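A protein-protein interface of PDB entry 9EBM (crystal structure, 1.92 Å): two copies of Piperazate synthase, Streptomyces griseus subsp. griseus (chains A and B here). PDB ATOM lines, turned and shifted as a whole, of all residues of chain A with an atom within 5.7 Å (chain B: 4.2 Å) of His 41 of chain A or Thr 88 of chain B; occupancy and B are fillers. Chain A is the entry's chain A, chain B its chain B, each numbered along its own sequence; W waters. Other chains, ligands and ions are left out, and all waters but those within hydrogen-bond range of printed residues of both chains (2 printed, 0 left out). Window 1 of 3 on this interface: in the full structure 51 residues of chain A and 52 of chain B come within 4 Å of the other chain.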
ATOM      1  N   LEU A  24     -14.830   1.526  27.754  1.00  0.00           N
ATOM      2  CA  LEU A  24     -13.386   1.565  27.512  1.00  0.00           C
ATOM      3  C   LEU A  24     -13.188   2.046  26.086  1.00  0.00           C
ATOM      4  O   LEU A  24     -13.247   1.256  25.143  1.00  0.00           O
ATOM      5  CB  LEU A  24     -12.740   0.205  27.722  1.00  0.00           C
ATOM      6  CG  LEU A  24     -11.200   0.288  27.793  1.00  0.00           C
ATOM      7  CD1 LEU A  24     -10.706   0.884  29.150  1.00  0.00           C
ATOM      8  CD2 LEU A  24     -10.551  -1.078  27.520  1.00  0.00           C
ATOM      9  N   ALA A  25     -12.969   3.347  25.921  1.00  0.00           N
ATOM     10  CA  ALA A  25     -12.892   3.935  24.591  1.00  0.00           C
ATOM     11  C   ALA A  25     -11.484   3.808  24.026  1.00  0.00           C
ATOM     12  O   ALA A  25     -10.514   3.598  24.752  1.00  0.00           O
ATOM     13  CB  ALA A  25     -13.284   5.404  24.645  1.00  0.00           C
ATOM     14  N   MET A  26     -11.379   3.924  22.710  1.00  0.00           N
ATOM     15  CA  MET A  26     -10.105   4.235  22.082  1.00  0.00           C
ATOM     16  C   MET A  26     -10.051   5.745  21.870  1.00  0.00           C
ATOM     17  O   MET A  26     -10.856   6.304  21.112  1.00  0.00           O
ATOM     18  CB  MET A  26      -9.917   3.478  20.767  1.00  0.00           C
ATOM     19  CG  MET A  26      -8.453   3.436  20.373  1.00  0.00           C
ATOM     20  SD  MET A  26      -8.038   2.329  19.012  1.00  0.00           S
ATOM     21  CE  MET A  26      -8.192   3.442  17.609  1.00  0.00           C
ATOM     22  N   ALA A  27      -9.112   6.400  22.548  1.00  0.00           N
ATOM     23  CA  ALA A  27      -8.976   7.848  22.507  1.00  0.00           C
ATOM     24  C   ALA A  27      -7.855   8.196  21.538  1.00  0.00           C
ATOM     25  O   ALA A  27      -6.716   7.746  21.710  1.00  0.00           O
ATOM     26  CB  ALA A  27      -8.683   8.401  23.904  1.00  0.00           C
ATOM     27  N   ALA A  39      -3.092   6.623  19.824  1.00  0.00           N
ATOM     28  CA  ALA A  39      -4.300   5.924  20.250  1.00  0.00           C
ATOM     29  C   ALA A  39      -4.032   5.210  21.564  1.00  0.00           C
ATOM     30  O   ALA A  39      -3.027   4.498  21.686  1.00  0.00           O
ATOM     31  CB  ALA A  39      -4.773   4.921  19.193  1.00  0.00           C
ATOM     32  N   THR A  40      -4.944   5.391  22.521  1.00  0.00           N
ATOM     33  CA  THR A  40      -4.874   4.805  23.857  1.00  0.00           C
ATOM     34  C   THR A  40      -6.260   4.314  24.262  1.00  0.00           C
ATOM     35  O   THR A  40      -7.254   5.030  24.096  1.00  0.00           O
ATOM     36  CB  THR A  40      -4.361   5.842  24.879  1.00  0.00           C
ATOM     37  OG1 THR A  40      -2.978   6.144  24.620  1.00  0.00           O
ATOM     38  CG2 THR A  40      -4.520   5.338  26.325  1.00  0.00           C
ATOM     39  N   HIS A  41      -6.335   3.103  24.808  1.00  0.00           N
ATOM     40  CA  HIS A  41      -7.597   2.583  25.338  1.00  0.00           C
ATOM     41  C   HIS A  41      -7.744   3.034  26.791  1.00  0.00           C
ATOM     42  O   HIS A  41      -6.882   2.717  27.612  1.00  0.00           O
ATOM     43  CB  HIS A  41      -7.606   1.058  25.234  1.00  0.00           C
ATOM     44  CG  HIS A  41      -7.483   0.550  23.825  1.00  0.00           C
ATOM     45  ND1 HIS A  41      -8.582   0.217  23.062  1.00  0.00           N
ATOM     46  CD2 HIS A  41      -6.399   0.322  23.042  1.00  0.00           C
ATOM     47  CE1 HIS A  41      -8.181  -0.200  21.870  1.00  0.00           C
ATOM     48  NE2 HIS A  41      -6.862  -0.135  21.828  1.00  0.00           N
ATOM     49  N   LEU A  42      -8.825   3.747  27.121  1.00  0.00           N
ATOM     50  CA  LEU A  42      -8.939   4.299  28.469  1.00  0.00           C
ATOM     51  C   LEU A  42     -10.411   4.443  28.859  1.00  0.00           C
ATOM     52  O   LEU A  42     -11.284   4.529  27.986  1.00  0.00           O
ATOM     53  CB  LEU A  42      -8.218   5.653  28.562  1.00  0.00           C
ATOM     54  CG  LEU A  42      -8.535   6.690  27.486  1.00  0.00           C
ATOM     55  CD1 LEU A  42      -9.814   7.467  27.804  1.00  0.00           C
ATOM     56  CD2 LEU A  42      -7.354   7.642  27.332  1.00  0.00           C
ATOM     57  N   PRO A  43     -10.720   4.513  30.160  1.00  0.00           N
ATOM     58  CA  PRO A  43     -12.132   4.553  30.571  1.00  0.00           C
ATOM     59  C   PRO A  43     -12.702   5.962  30.499  1.00  0.00           C
ATOM     60  O   PRO A  43     -12.065   6.934  30.915  1.00  0.00           O
ATOM     61  CB  PRO A  43     -12.098   4.042  32.020  1.00  0.00           C
ATOM     62  CG  PRO A  43     -10.739   4.551  32.549  1.00  0.00           C
ATOM     63  CD  PRO A  43      -9.804   4.450  31.324  1.00  0.00           C
ATOM     64  N   THR A  88     -17.010   0.797  20.904  1.00  0.00           N
ATOM     65  CA  THR A  88     -17.538  -0.289  20.087  1.00  0.00           C
ATOM     66  C   THR A  88     -18.364  -1.218  20.963  1.00  0.00           C
ATOM     67  O   THR A  88     -18.000  -1.484  22.114  1.00  0.00           O
ATOM     68  CB  THR A  88     -16.404  -1.076  19.405  1.00  0.00           C
ATOM     69  OG1 THR A  88     -15.519  -1.594  20.405  1.00  0.00           O
ATOM     70  CG2 THR A  88     -15.606  -0.167  18.457  1.00  0.00           C
ATOM     71  N   LEU B  18      -5.007 -12.672  17.702  1.00  0.00           N
ATOM     72  CA  LEU B  18      -6.050 -11.688  17.965  1.00  0.00           C
ATOM     73  C   LEU B  18      -6.564 -11.063  16.665  1.00  0.00           C
ATOM     74  O   LEU B  18      -7.774 -10.904  16.474  1.00  0.00           O
ATOM     75  CB  LEU B  18      -5.533 -10.607  18.904  1.00  0.00           C
ATOM     76  CG  LEU B  18      -6.661  -9.707  19.407  1.00  0.00           C
ATOM     77  CD1 LEU B  18      -6.408  -9.292  20.836  1.00  0.00           C
ATOM     78  CD2 LEU B  18      -6.803  -8.460  18.552  1.00  0.00           C
ATOM     79  N   ASN B  22     -10.407 -11.232  15.232  1.00  0.00           N
ATOM     80  CA  ASN B  22     -11.103  -9.948  15.305  1.00  0.00           C
ATOM     81  C   ASN B  22     -10.612  -9.040  14.187  1.00  0.00           C
ATOM     82  O   ASN B  22     -10.058  -7.967  14.434  1.00  0.00           O
ATOM     83  CB  ASN B  22     -10.883  -9.303  16.673  1.00  0.00           C
ATOM     84  CG  ASN B  22     -11.155 -10.269  17.797  1.00  0.00           C
ATOM     85  OD1 ASN B  22     -12.294 -10.408  18.230  1.00  0.00           O
ATOM     86  ND2 ASN B  22     -10.119 -10.999  18.233  1.00  0.00           N
ATOM     87  N   PHE B  87      -6.866  -3.421  16.348  1.00  0.00           N
ATOM     88  CA  PHE B  87      -7.691  -4.609  16.538  1.00  0.00           C
ATOM     89  C   PHE B  87      -7.912  -4.829  18.031  1.00  0.00           C
ATOM     90  O   PHE B  87      -6.973  -4.687  18.821  1.00  0.00           O
ATOM     91  CB  PHE B  87      -7.003  -5.841  15.956  1.00  0.00           C
ATOM     92  CG  PHE B  87      -6.602  -5.705  14.513  1.00  0.00           C
ATOM     93  CD1 PHE B  87      -5.403  -5.098  14.157  1.00  0.00           C
ATOM     94  CD2 PHE B  87      -7.425  -6.200  13.511  1.00  0.00           C
ATOM     95  CE1 PHE B  87      -5.026  -4.987  12.813  1.00  0.00           C
ATOM     96  CE2 PHE B  87      -7.063  -6.088  12.175  1.00  0.00           C
ATOM     97  CZ  PHE B  87      -5.863  -5.482  11.826  1.00  0.00           C
ATOM     98  N   THR B  88      -9.134  -5.196  18.415  1.00  0.00           N
ATOM     99  CA  THR B  88      -9.479  -5.433  19.816  1.00  0.00           C
ATOM    100  C   THR B  88     -10.097  -6.816  19.986  1.00  0.00           C
ATOM    101  O   THR B  88     -10.845  -7.286  19.126  1.00  0.00           O
ATOM    102  CB  THR B  88     -10.455  -4.395  20.327  1.00  0.00           C
ATOM    103  OG1 THR B  88     -11.554  -4.314  19.413  1.00  0.00           O
ATOM    104  CG2 THR B  88      -9.779  -3.043  20.421  1.00  0.00           C
ATOM    105  N   GLY B  89      -9.782  -7.471  21.097  1.00  0.00           N
ATOM    106  CA  GLY B  89     -10.382  -8.747  21.408  1.00  0.00           C
ATOM    107  C   GLY B  89     -11.142  -8.729  22.727  1.00  0.00           C
ATOM    108  O   GLY B  89     -11.736  -7.717  23.124  1.00  0.00           O
ATOM    109  N   PHE B 110      -8.217  -5.993  29.109  1.00  0.00           N
ATOM    110  CA  PHE B 110      -8.609  -5.915  27.704  1.00  0.00           C
ATOM    111  C   PHE B 110      -7.453  -6.342  26.821  1.00  0.00           C
ATOM    112  O   PHE B 110      -6.304  -6.457  27.261  1.00  0.00           O
ATOM    113  CB  PHE B 110      -9.088  -4.501  27.339  1.00  0.00           C
ATOM    114  CG  PHE B 110      -7.986  -3.485  27.260  1.00  0.00           C
ATOM    115  CD1 PHE B 110      -7.548  -2.832  28.407  1.00  0.00           C
ATOM    116  CD2 PHE B 110      -7.412  -3.155  26.038  1.00  0.00           C
ATOM    117  CE1 PHE B 110      -6.546  -1.874  28.338  1.00  0.00           C
ATOM    118  CE2 PHE B 110      -6.408  -2.215  25.964  1.00  0.00           C
ATOM    119  CZ  PHE B 110      -5.975  -1.567  27.118  1.00  0.00           C
ATOM    120  N   THR B 111      -7.767  -6.550  25.542  1.00  0.00           N
ATOM    121  CA  THR B 111      -6.760  -6.959  24.585  1.00  0.00           C
ATOM    122  C   THR B 111      -6.824  -6.067  23.349  1.00  0.00           C
ATOM    123  O   THR B 111      -7.910  -5.710  22.875  1.00  0.00           O
ATOM    124  CB  THR B 111      -6.941  -8.425  24.198  1.00  0.00           C
ATOM    125  OG1 THR B 111      -8.277  -8.625  23.718  1.00  0.00           O
ATOM    126  CG2 THR B 111      -6.688  -9.328  25.416  1.00  0.00           C
ATOM    127  N   SER B 112      -5.654  -5.698  22.841  1.00  0.00           N
ATOM    128  CA  SER B 112      -5.602  -4.822  21.678  1.00  0.00           C
ATOM    129  C   SER B 112      -4.288  -5.035  20.951  1.00  0.00           C
ATOM    130  O   SER B 112      -3.257  -5.295  21.581  1.00  0.00           O
ATOM    131  CB  SER B 112      -5.763  -3.349  22.085  1.00  0.00           C
ATOM    132  OG  SER B 112      -5.798  -2.505  20.949  1.00  0.00           O
ATOM    133  N   HIS B 114      -2.159  -2.895  18.017  1.00  0.00           N
ATOM    134  CA  HIS B 114      -2.017  -1.725  17.170  1.00  0.00           C
ATOM    135  C   HIS B 114      -0.964  -2.030  16.116  1.00  0.00           C
ATOM    136  O   HIS B 114       0.203  -2.291  16.441  1.00  0.00           O
ATOM    137  CB  HIS B 114      -1.625  -0.487  17.980  1.00  0.00           C
ATOM    138  CG  HIS B 114      -2.742   0.077  18.792  1.00  0.00           C
ATOM    139  ND1 HIS B 114      -2.640   1.276  19.469  1.00  0.00           N
ATOM    140  CD2 HIS B 114      -3.987  -0.396  19.045  1.00  0.00           C
ATOM    141  CE1 HIS B 114      -3.777   1.518  20.098  1.00  0.00           C
ATOM    142  NE2 HIS B 114      -4.607   0.518  19.864  1.00  0.00           N
HETATM  143  O   HOH W   1     -12.988  -1.740  19.625  1.00  0.00           O
HETATM  144  O   HOH W   2     -14.839  -4.534  18.818  1.00  0.00           O
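The side-chain hydroxyl of Ser 112 of chain B lies within hydrogen-bond range of a ring nitrogen (NE2) of His 41 of chain A. NE2 of His 114 of chain B sits at hydrogen-bond distance from NE2 of His 41 of chain A (3.1 Å).
O of Phe 87 of chain B sits close to OG of Ser 112 of chain B, at 3.3 Å. The side-chain hydroxyl (OG) of Ser 112 of chain B sits close to a ring nitrogen (NE2) of His 114 of chain B (3.4 Å).
Among the printed residues, merely in contact across the chains: Ala 39 of chain A with His 114 of chain B (3.5 Å), Leu 24 of chain A with Phe 110 of chain B (3.5 Å), His 41 of chain A with Phe 110 of chain B (3.6 Å), His 41 of chain A with Thr 88 of chain B (3.6 Å) and Met 26 of chain A with His 114 of chain B (3.97 Å).
Of the printed residues of chain B, Leu 24 of chain A touches Phe 110 (3.5 Å). Of the printed residues of chain B, Met 26 of chain A touches His 114. Of the printed residues of chain B, Ala 39 of chain A touches His 114 (3.5 Å). His 41 of chain A touches four residues of chain B. Printed residues of chain A within 4 Å of Thr 88 of chain B: His 41 (3.6 Å). The nearest residue of chain A that does not touch Thr 88 of chain B is Thr 88 of chain A (4.9 Å).
Of the 10 printed residues of chain A, 4 touch a printed residue of chain B. Hydrophobic or aromatic side chains of chain A within 4 Å of the printed part of chain B: Leu 24, Met 26, Ala 39 and His 41. Printed residues of chain B that touch a printed residue of chain A: Thr 88, Phe 110, Ser 112 and His 114. Hydrophobic or aromatic side chains of chain B within 4 Å of the printed part of chain A: Phe 110 and His 114. Among the printed residues, 7 pairs touch across the chains.
Position printed for both chains: 88.
Water W1 lies within hydrogen-bond range of the side-chain hydroxyl (OG1) of Thr 88 of chain A and the side-chain hydroxyl (OG1) of Thr 88 of chain B. Water W2 lies within hydrogen-bond range of the side-chain hydroxyl of Thr 88 of chain B (3.3 Å) and the side-chain hydroxyl of Thr 88 of chain A (3.4 Å).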
